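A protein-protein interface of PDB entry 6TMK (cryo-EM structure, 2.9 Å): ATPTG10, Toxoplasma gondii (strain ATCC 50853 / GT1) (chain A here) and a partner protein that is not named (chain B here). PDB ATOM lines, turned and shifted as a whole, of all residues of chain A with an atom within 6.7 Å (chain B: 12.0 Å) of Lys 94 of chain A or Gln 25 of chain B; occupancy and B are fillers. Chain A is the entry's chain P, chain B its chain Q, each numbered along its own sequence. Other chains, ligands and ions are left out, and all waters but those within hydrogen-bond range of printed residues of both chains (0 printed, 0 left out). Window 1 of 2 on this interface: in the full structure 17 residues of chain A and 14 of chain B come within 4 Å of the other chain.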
ATOM      1  N   TYR A  32       4.844  19.788  -1.158  1.00  0.00           N
ATOM      2  CA  TYR A  32       3.689  18.902  -1.108  1.00  0.00           C
ATOM      3  C   TYR A  32       4.091  17.471  -1.425  1.00  0.00           C
ATOM      4  O   TYR A  32       3.692  16.531  -0.729  1.00  0.00           O
ATOM      5  CB  TYR A  32       2.622  19.397  -2.081  1.00  0.00           C
ATOM      6  CG  TYR A  32       1.253  18.813  -1.859  1.00  0.00           C
ATOM      7  CD1 TYR A  32       0.357  19.408  -0.992  1.00  0.00           C
ATOM      8  CD2 TYR A  32       0.848  17.678  -2.535  1.00  0.00           C
ATOM      9  CE1 TYR A  32      -0.895  18.880  -0.793  1.00  0.00           C
ATOM     10  CE2 TYR A  32      -0.400  17.145  -2.342  1.00  0.00           C
ATOM     11  CZ  TYR A  32      -1.270  17.751  -1.473  1.00  0.00           C
ATOM     12  OH  TYR A  32      -2.521  17.221  -1.277  1.00  0.00           O
ATOM     13  N   MET A  44       1.597  19.214   4.291  1.00  0.00           N
ATOM     14  CA  MET A  44       1.094  19.315   2.929  1.00  0.00           C
ATOM     15  C   MET A  44      -0.145  20.202   2.846  1.00  0.00           C
ATOM     16  O   MET A  44      -0.354  20.871   1.827  1.00  0.00           O
ATOM     17  CB  MET A  44       0.821  17.924   2.377  1.00  0.00           C
ATOM     18  CG  MET A  44      -0.273  17.182   3.062  1.00  0.00           C
ATOM     19  SD  MET A  44       0.087  15.418   3.030  1.00  0.00           S
ATOM     20  CE  MET A  44       0.018  15.121   1.279  1.00  0.00           C
ATOM     21  N   GLU A  45      -0.943  20.283   3.913  1.00  0.00           N
ATOM     22  CA  GLU A  45      -2.059  21.220   3.901  1.00  0.00           C
ATOM     23  C   GLU A  45      -1.565  22.653   4.033  1.00  0.00           C
ATOM     24  O   GLU A  45      -2.130  23.568   3.423  1.00  0.00           O
ATOM     25  CB  GLU A  45      -3.056  20.888   5.009  1.00  0.00           C
ATOM     26  CG  GLU A  45      -2.565  21.157   6.412  1.00  0.00           C
ATOM     27  CD  GLU A  45      -3.658  21.005   7.452  1.00  0.00           C
ATOM     28  OE1 GLU A  45      -4.840  21.215   7.111  1.00  0.00           O
ATOM     29  OE2 GLU A  45      -3.334  20.681   8.615  1.00  0.00           O
ATOM     30  N   PHE A  48      -0.558  23.515   0.568  1.00  0.00           N
ATOM     31  CA  PHE A  48      -1.722  23.799  -0.261  1.00  0.00           C
ATOM     32  C   PHE A  48      -2.293  25.178   0.043  1.00  0.00           C
ATOM     33  O   PHE A  48      -2.691  25.911  -0.869  1.00  0.00           O
ATOM     34  CB  PHE A  48      -2.782  22.723  -0.038  1.00  0.00           C
ATOM     35  CG  PHE A  48      -3.947  22.819  -0.966  1.00  0.00           C
ATOM     36  CD1 PHE A  48      -3.881  22.284  -2.231  1.00  0.00           C
ATOM     37  CD2 PHE A  48      -5.112  23.442  -0.570  1.00  0.00           C
ATOM     38  CE1 PHE A  48      -4.948  22.369  -3.082  1.00  0.00           C
ATOM     39  CE2 PHE A  48      -6.182  23.526  -1.420  1.00  0.00           C
ATOM     40  CZ  PHE A  48      -6.100  22.989  -2.677  1.00  0.00           C
ATOM     41  N   TRP A  53      -3.344  31.656  -3.998  1.00  0.00           N
ATOM     42  CA  TRP A  53      -4.675  31.613  -4.590  1.00  0.00           C
ATOM     43  C   TRP A  53      -5.279  32.991  -4.812  1.00  0.00           C
ATOM     44  O   TRP A  53      -6.340  33.085  -5.437  1.00  0.00           O
ATOM     45  CB  TRP A  53      -5.613  30.797  -3.714  1.00  0.00           C
ATOM     46  CG  TRP A  53      -5.159  29.410  -3.461  1.00  0.00           C
ATOM     47  CD1 TRP A  53      -4.570  28.933  -2.333  1.00  0.00           C
ATOM     48  CD2 TRP A  53      -5.263  28.306  -4.357  1.00  0.00           C
ATOM     49  NE1 TRP A  53      -4.300  27.596  -2.470  1.00  0.00           N
ATOM     50  CE2 TRP A  53      -4.716  27.188  -3.708  1.00  0.00           C
ATOM     51  CE3 TRP A  53      -5.766  28.154  -5.648  1.00  0.00           C
ATOM     52  CZ2 TRP A  53      -4.658  25.940  -4.306  1.00  0.00           C
ATOM     53  CZ3 TRP A  53      -5.705  26.916  -6.236  1.00  0.00           C
ATOM     54  CH2 TRP A  53      -5.158  25.826  -5.567  1.00  0.00           C
ATOM     55  N   LYS A  91      -8.500  11.400  -9.148  1.00  0.00           N
ATOM     56  CA  LYS A  91      -9.435  11.410  -8.038  1.00  0.00           C
ATOM     57  C   LYS A  91      -9.087  12.435  -6.967  1.00  0.00           C
ATOM     58  O   LYS A  91      -9.934  12.725  -6.117  1.00  0.00           O
ATOM     59  CB  LYS A  91      -9.505  10.023  -7.406  1.00  0.00           C
ATOM     60  CG  LYS A  91      -9.826   8.930  -8.392  1.00  0.00           C
ATOM     61  CD  LYS A  91      -9.926   7.584  -7.718  1.00  0.00           C
ATOM     62  CE  LYS A  91     -10.412   6.522  -8.685  1.00  0.00           C
ATOM     63  NZ  LYS A  91     -11.783   6.802  -9.202  1.00  0.00           N
ATOM     64  N   ASP A  92      -7.870  12.986  -6.978  1.00  0.00           N
ATOM     65  CA  ASP A  92      -7.415  13.833  -5.887  1.00  0.00           C
ATOM     66  C   ASP A  92      -7.628  15.297  -6.246  1.00  0.00           C
ATOM     67  O   ASP A  92      -6.863  15.859  -7.054  1.00  0.00           O
ATOM     68  CB  ASP A  92      -5.941  13.564  -5.580  1.00  0.00           C
ATOM     69  CG  ASP A  92      -5.505  14.148  -4.254  1.00  0.00           C
ATOM     70  OD1 ASP A  92      -5.717  15.358  -4.036  1.00  0.00           O
ATOM     71  OD2 ASP A  92      -4.944  13.397  -3.429  1.00  0.00           O
ATOM     72  N   PRO A  93      -8.634  15.964  -5.674  1.00  0.00           N
ATOM     73  CA  PRO A  93      -8.972  17.302  -6.159  1.00  0.00           C
ATOM     74  C   PRO A  93      -7.931  18.337  -5.803  1.00  0.00           C
ATOM     75  O   PRO A  93      -7.786  19.320  -6.534  1.00  0.00           O
ATOM     76  CB  PRO A  93     -10.316  17.586  -5.477  1.00  0.00           C
ATOM     77  CG  PRO A  93     -10.297  16.754  -4.270  1.00  0.00           C
ATOM     78  CD  PRO A  93      -9.584  15.508  -4.648  1.00  0.00           C
ATOM     79  N   LYS A  94      -7.200  18.158  -4.706  1.00  0.00           N
ATOM     80  CA  LYS A  94      -6.163  19.119  -4.352  1.00  0.00           C
ATOM     81  C   LYS A  94      -5.068  19.144  -5.409  1.00  0.00           C
ATOM     82  O   LYS A  94      -4.640  20.213  -5.867  1.00  0.00           O
ATOM     83  CB  LYS A  94      -5.589  18.773  -2.984  1.00  0.00           C
ATOM     84  CG  LYS A  94      -6.392  19.309  -1.830  1.00  0.00           C
ATOM     85  CD  LYS A  94      -5.910  18.744  -0.519  1.00  0.00           C
ATOM     86  CE  LYS A  94      -6.204  19.674   0.636  1.00  0.00           C
ATOM     87  NZ  LYS A  94      -7.578  20.211   0.581  1.00  0.00           N
ATOM     88  N   GLN A  95      -4.599  17.960  -5.802  1.00  0.00           N
ATOM     89  CA  GLN A  95      -3.631  17.845  -6.884  1.00  0.00           C
ATOM     90  C   GLN A  95      -4.186  18.433  -8.173  1.00  0.00           C
ATOM     91  O   GLN A  95      -3.502  19.190  -8.875  1.00  0.00           O
ATOM     92  CB  GLN A  95      -3.268  16.378  -7.076  1.00  0.00           C
ATOM     93  CG  GLN A  95      -2.320  15.835  -6.034  1.00  0.00           C
ATOM     94  CD  GLN A  95      -2.100  14.347  -6.175  1.00  0.00           C
ATOM     95  OE1 GLN A  95      -2.939  13.544  -5.771  1.00  0.00           O
ATOM     96  NE2 GLN A  95      -0.969  13.968  -6.747  1.00  0.00           N
ATOM     97  N   THR A  96      -5.431  18.082  -8.506  1.00  0.00           N
ATOM     98  CA  THR A  96      -6.046  18.618  -9.715  1.00  0.00           C
ATOM     99  C   THR A  96      -6.056  20.140  -9.697  1.00  0.00           C
ATOM    100  O   THR A  96      -5.757  20.789 -10.708  1.00  0.00           O
ATOM    101  CB  THR A  96      -7.464  18.075  -9.860  1.00  0.00           C
ATOM    102  OG1 THR A  96      -7.417  16.657 -10.052  1.00  0.00           O
ATOM    103  CG2 THR A  96      -8.159  18.714 -11.036  1.00  0.00           C
ATOM    104  N   LEU A  97      -6.379  20.727  -8.547  1.00  0.00           N
ATOM    105  CA  LEU A  97      -6.522  22.171  -8.456  1.00  0.00           C
ATOM    106  C   LEU A  97      -5.175  22.863  -8.551  1.00  0.00           C
ATOM    107  O   LEU A  97      -5.057  23.915  -9.188  1.00  0.00           O
ATOM    108  CB  LEU A  97      -7.213  22.534  -7.150  1.00  0.00           C
ATOM    109  CG  LEU A  97      -8.682  22.144  -7.052  1.00  0.00           C
ATOM    110  CD1 LEU A  97      -9.094  22.139  -5.609  1.00  0.00           C
ATOM    111  CD2 LEU A  97      -9.551  23.063  -7.856  1.00  0.00           C
ATOM    112  N   MET A  98      -4.151  22.309  -7.904  1.00  0.00           N
ATOM    113  CA  MET A  98      -2.826  22.906  -8.016  1.00  0.00           C
ATOM    114  C   MET A  98      -2.313  22.826  -9.447  1.00  0.00           C
ATOM    115  O   MET A  98      -1.681  23.768  -9.945  1.00  0.00           O
ATOM    116  CB  MET A  98      -1.866  22.225  -7.053  1.00  0.00           C
ATOM    117  CG  MET A  98      -2.185  22.507  -5.609  1.00  0.00           C
ATOM    118  SD  MET A  98      -0.827  22.143  -4.494  1.00  0.00           S
ATOM    119  CE  MET A  98      -0.862  20.364  -4.563  1.00  0.00           C
ATOM    120  N   SER A  99      -2.582  21.713 -10.130  1.00  0.00           N
ATOM    121  CA  SER A  99      -2.243  21.616 -11.544  1.00  0.00           C
ATOM    122  C   SER A  99      -2.946  22.700 -12.350  1.00  0.00           C
ATOM    123  O   SER A  99      -2.328  23.371 -13.185  1.00  0.00           O
ATOM    124  CB  SER A  99      -2.608  20.230 -12.066  1.00  0.00           C
ATOM    125  OG  SER A  99      -2.071  19.224 -11.230  1.00  0.00           O
ATOM    126  N   VAL B  21      -2.884   4.810   5.957  1.00  0.00           N
ATOM    127  CA  VAL B  21      -2.485   5.929   5.102  1.00  0.00           C
ATOM    128  C   VAL B  21      -3.378   7.126   5.419  1.00  0.00           C
ATOM    129  O   VAL B  21      -4.609   6.977   5.434  1.00  0.00           O
ATOM    130  CB  VAL B  21      -2.584   5.543   3.633  1.00  0.00           C
ATOM    131  CG1 VAL B  21      -2.446   6.768   2.757  1.00  0.00           C
ATOM    132  CG2 VAL B  21      -1.509   4.540   3.289  1.00  0.00           C
ATOM    133  N   PRO B  22      -2.818   8.310   5.673  1.00  0.00           N
ATOM    134  CA  PRO B  22      -3.666   9.441   6.067  1.00  0.00           C
ATOM    135  C   PRO B  22      -4.630   9.877   4.976  1.00  0.00           C
ATOM    136  O   PRO B  22      -4.604   9.360   3.856  1.00  0.00           O
ATOM    137  CB  PRO B  22      -2.652  10.549   6.381  1.00  0.00           C
ATOM    138  CG  PRO B  22      -1.374   9.856   6.610  1.00  0.00           C
ATOM    139  CD  PRO B  22      -1.390   8.656   5.738  1.00  0.00           C
ATOM    140  N   PHE B  23      -5.485  10.842   5.306  1.00  0.00           N
ATOM    141  CA  PHE B  23      -6.464  11.389   4.377  1.00  0.00           C
ATOM    142  C   PHE B  23      -6.453  12.898   4.542  1.00  0.00           C
ATOM    143  O   PHE B  23      -6.747  13.400   5.629  1.00  0.00           O
ATOM    144  CB  PHE B  23      -7.858  10.818   4.644  1.00  0.00           C
ATOM    145  CG  PHE B  23      -8.902  11.287   3.682  1.00  0.00           C
ATOM    146  CD1 PHE B  23      -9.126  10.606   2.503  1.00  0.00           C
ATOM    147  CD2 PHE B  23      -9.671  12.400   3.962  1.00  0.00           C
ATOM    148  CE1 PHE B  23     -10.089  11.033   1.618  1.00  0.00           C
ATOM    149  CE2 PHE B  23     -10.634  12.828   3.080  1.00  0.00           C
ATOM    150  CZ  PHE B  23     -10.842  12.145   1.908  1.00  0.00           C
ATOM    151  N   VAL B  24      -6.115  13.618   3.474  1.00  0.00           N
ATOM    152  CA  VAL B  24      -5.787  15.035   3.569  1.00  0.00           C
ATOM    153  C   VAL B  24      -6.776  15.924   2.842  1.00  0.00           C
ATOM    154  O   VAL B  24      -6.636  17.154   2.901  1.00  0.00           O
ATOM    155  CB  VAL B  24      -4.359  15.302   3.062  1.00  0.00           C
ATOM    156  CG1 VAL B  24      -3.397  14.370   3.741  1.00  0.00           C
ATOM    157  CG2 VAL B  24      -4.286  15.125   1.564  1.00  0.00           C
ATOM    158  N   GLN B  25      -7.773  15.359   2.163  1.00  0.00           N
ATOM    159  CA  GLN B  25      -8.756  16.207   1.501  1.00  0.00           C
ATOM    160  C   GLN B  25      -9.607  16.952   2.519  1.00  0.00           C
ATOM    161  O   GLN B  25      -9.989  18.105   2.294  1.00  0.00           O
ATOM    162  CB  GLN B  25      -9.637  15.370   0.581  1.00  0.00           C
ATOM    163  CG  GLN B  25      -8.882  14.486  -0.385  1.00  0.00           C
ATOM    164  CD  GLN B  25      -7.916  15.258  -1.246  1.00  0.00           C
ATOM    165  OE1 GLN B  25      -8.262  16.291  -1.814  1.00  0.00           O
ATOM    166  NE2 GLN B  25      -6.698  14.758  -1.356  1.00  0.00           N
ATOM    167  N   PHE B  26      -9.919  16.308   3.639  1.00  0.00           N
ATOM    168  CA  PHE B  26     -10.646  16.950   4.724  1.00  0.00           C
ATOM    169  C   PHE B  26     -10.511  16.086   5.972  1.00  0.00           C
ATOM    170  O   PHE B  26      -9.942  14.992   5.937  1.00  0.00           O
ATOM    171  CB  PHE B  26     -12.105  17.194   4.335  1.00  0.00           C
ATOM    172  CG  PHE B  26     -12.758  16.030   3.660  1.00  0.00           C
ATOM    173  CD1 PHE B  26     -12.786  15.948   2.285  1.00  0.00           C
ATOM    174  CD2 PHE B  26     -13.351  15.025   4.394  1.00  0.00           C
ATOM    175  CE1 PHE B  26     -13.383  14.886   1.655  1.00  0.00           C
ATOM    176  CE2 PHE B  26     -13.953  13.959   3.766  1.00  0.00           C
ATOM    177  CZ  PHE B  26     -13.967  13.891   2.394  1.00  0.00           C
ATOM    178  N   ASP B  27     -11.050  16.593   7.082  1.00  0.00           N
ATOM    179  CA  ASP B  27     -10.788  15.985   8.385  1.00  0.00           C
ATOM    180  C   ASP B  27     -11.328  14.562   8.459  1.00  0.00           C
ATOM    181  O   ASP B  27     -10.673  13.669   9.011  1.00  0.00           O
ATOM    182  CB  ASP B  27     -11.397  16.847   9.488  1.00  0.00           C
ATOM    183  CG  ASP B  27     -10.943  16.430  10.869  1.00  0.00           C
ATOM    184  OD1 ASP B  27     -10.436  17.292  11.614  1.00  0.00           O
ATOM    185  OD2 ASP B  27     -11.093  15.238  11.212  1.00  0.00           O
ATOM    186  N   GLN B  28     -12.527  14.335   7.926  1.00  0.00           N
ATOM    187  CA  GLN B  28     -13.241  13.060   7.921  1.00  0.00           C
ATOM    188  C   GLN B  28     -13.740  12.635   9.298  1.00  0.00           C
ATOM    189  O   GLN B  28     -14.423  11.609   9.395  1.00  0.00           O
ATOM    190  CB  GLN B  28     -12.395  11.911   7.355  1.00  0.00           C
ATOM    191  CG  GLN B  28     -12.640  11.633   5.895  1.00  0.00           C
ATOM    192  CD  GLN B  28     -12.055  10.312   5.456  1.00  0.00           C
ATOM    193  OE1 GLN B  28     -11.052   9.851   6.002  1.00  0.00           O
ATOM    194  NE2 GLN B  28     -12.683   9.687   4.473  1.00  0.00           N
ATOM    195  N   THR B  29     -13.434  13.377  10.360  1.00  0.00           N
ATOM    196  CA  THR B  29     -13.941  13.064  11.688  1.00  0.00           C
ATOM    197  C   THR B  29     -15.097  13.963  12.100  1.00  0.00           C
ATOM    198  O   THR B  29     -15.609  13.817  13.212  1.00  0.00           O
ATOM    199  CB  THR B  29     -12.821  13.171  12.729  1.00  0.00           C
ATOM    200  OG1 THR B  29     -12.444  14.542  12.893  1.00  0.00           O
ATOM    201  CG2 THR B  29     -11.613  12.357  12.299  1.00  0.00           C
ATOM    202  N   ALA B  30     -15.518  14.878  11.238  1.00  0.00           N
ATOM    203  CA  ALA B  30     -16.526  15.872  11.554  1.00  0.00           C
ATOM    204  C   ALA B  30     -17.683  15.760  10.573  1.00  0.00           C
ATOM    205  O   ALA B  30     -17.551  15.140   9.512  1.00  0.00           O
ATOM    206  CB  ALA B  30     -15.936  17.289  11.499  1.00  0.00           C
ATOM    207  N   PRO B  31     -18.834  16.348  10.892  1.00  0.00           N
ATOM    208  CA  PRO B  31     -19.956  16.307   9.952  1.00  0.00           C
ATOM    209  C   PRO B  31     -19.650  17.064   8.671  1.00  0.00           C
ATOM    210  O   PRO B  31     -18.772  17.928   8.615  1.00  0.00           O
ATOM    211  CB  PRO B  31     -21.100  16.973  10.730  1.00  0.00           C
ATOM    212  CG  PRO B  31     -20.690  16.910  12.160  1.00  0.00           C
ATOM    213  CD  PRO B  31     -19.202  17.005  12.155  1.00  0.00           C
ATOM    214  N   SER B  32     -20.396  16.726   7.634  1.00  0.00           N
ATOM    215  CA  SER B  32     -20.279  17.394   6.346  1.00  0.00           C
ATOM    216  C   SER B  32     -21.228  18.586   6.296  1.00  0.00           C
ATOM    217  O   SER B  32     -22.421  18.425   6.576  1.00  0.00           O
ATOM    218  CB  SER B  32     -20.599  16.435   5.212  1.00  0.00           C
ATOM    219  OG  SER B  32     -19.810  15.262   5.308  1.00  0.00           O
ATOM    220  N   PRO B  33     -20.760  19.786   5.954  1.00  0.00           N
ATOM    221  CA  PRO B  33     -21.696  20.903   5.778  1.00  0.00           C
ATOM    222  C   PRO B  33     -22.571  20.676   4.556  1.00  0.00           C
ATOM    223  O   PRO B  33     -22.079  20.323   3.482  1.00  0.00           O
ATOM    224  CB  PRO B  33     -20.778  22.120   5.600  1.00  0.00           C
ATOM    225  CG  PRO B  33     -19.445  21.685   6.095  1.00  0.00           C
ATOM    226  CD  PRO B  33     -19.364  20.225   5.814  1.00  0.00           C
ATOM    227  N   LEU B 108     -24.722  16.064  -1.652  1.00  0.00           N
ATOM    228  CA  LEU B 108     -23.974  14.813  -1.674  1.00  0.00           C
ATOM    229  C   LEU B 108     -24.761  13.699  -2.345  1.00  0.00           C
ATOM    230  O   LEU B 108     -24.169  12.780  -2.918  1.00  0.00           O
ATOM    231  CB  LEU B 108     -23.602  14.405  -0.252  1.00  0.00           C
ATOM    232  CG  LEU B 108     -22.801  15.425   0.552  1.00  0.00           C
ATOM    233  CD1 LEU B 108     -23.002  15.202   2.036  1.00  0.00           C
ATOM    234  CD2 LEU B 108     -21.331  15.347   0.197  1.00  0.00           C
ATOM    235  N   TYR B 122      -7.475   7.999 -17.934  1.00  0.00           N
ATOM    236  CA  TYR B 122      -6.466   8.707 -18.706  1.00  0.00           C
ATOM    237  C   TYR B 122      -6.435   8.192 -20.138  1.00  0.00           C
ATOM    238  O   TYR B 122      -6.682   7.013 -20.406  1.00  0.00           O
ATOM    239  CB  TYR B 122      -5.088   8.537 -18.076  1.00  0.00           C
ATOM    240  CG  TYR B 122      -4.695   9.627 -17.112  1.00  0.00           C
ATOM    241  CD1 TYR B 122      -4.003  10.740 -17.549  1.00  0.00           C
ATOM    242  CD2 TYR B 122      -5.002   9.537 -15.766  1.00  0.00           C
ATOM    243  CE1 TYR B 122      -3.636  11.735 -16.680  1.00  0.00           C
ATOM    244  CE2 TYR B 122      -4.636  10.530 -14.890  1.00  0.00           C
ATOM    245  CZ  TYR B 122      -3.953  11.626 -15.351  1.00  0.00           C
ATOM    246  OH  TYR B 122      -3.589  12.615 -14.473  1.00  0.00           O
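The side-chain amide nitrogen of Gln 25 of chain B lies within hydrogen-bond range of the side-chain carboxylate of Asp 92 of chain A, 2.9 Å away.
OD1 of Asp 92 of chain A lies within hydrogen-bond range of N of Lys 94 of chain A, 3.2 Å away. The side-chain amide oxygen (OE1) of Gln 95 of chain A lies close to the side-chain carboxylate (OD2) of Asp 92 of chain A (3.1 Å). The side-chain hydroxyl (OG1) of Thr 96 of chain A lies within hydrogen-bond range of the backbone carbonyl oxygen (O) of Asp 92 of chain A (3.2 Å).
Among the printed residues, pairs that only touch across the chains: Pro 93 of chain A with Gln 25 of chain B, Lys 94 of chain A with Val 24 of chain B, Lys 94 of chain A with Gln 25 of chain B, Met 44 of chain A with Val 24 of chain B and Tyr 32 of chain A with Val 24 of chain B.
Printed residues of chain B within 4 Å of Lys 94 of chain A: Val 24 and Gln 25. Gln 25 of chain B touches just these residues of chain A: Asp 92, Pro 93 and Lys 94. No residue of chain B comes within 4 Å of Phe 48 of chain A. Printed residues of chain B within 4 Å of Asp 92 of chain A: Gln 25. Pro 93 of chain A touches just one residue of chain B: Gln 25. No residue of chain B comes within 4 Å of Leu 97 of chain A. No residue of chain B comes within 4 Å of Met 98 of chain A. Of the printed residues of chain B, Met 44 of chain A touches Val 24 (3.7 Å). Of the printed residues of chain A, Val 24 of chain B touches Tyr 32 (3.9 Å), Met 44 (3.7 Å) and Lys 94 (3.4 Å). Of the printed residues of chain B, Tyr 32 of chain A touches Val 24 (3.9 Å). Ala 30 of chain B touches none of the printed residues of chain A. Tyr 122 of chain B touches none of the printed residues of chain A. The nearest residue of chain B that does not touch Lys 94 of chain A is Phe 26 of chain B (5.5 Å). The nearest residue of chain A that does not touch Gln 25 of chain B is Tyr 32 of chain A (4.8 Å).
Hydrophobic or aromatic side chains of chain A within 4 Å of the printed part of chain B: Tyr 32, Met 44 and Pro 93. Of the 15 printed residues of chain B, 2 touch a printed residue of chain A. Printed residues of chain B that touch a printed residue of chain A: Val 24 and Gln 25. Along chain B the printed residues that touch a printed residue of chain A span positions 24 to 25.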
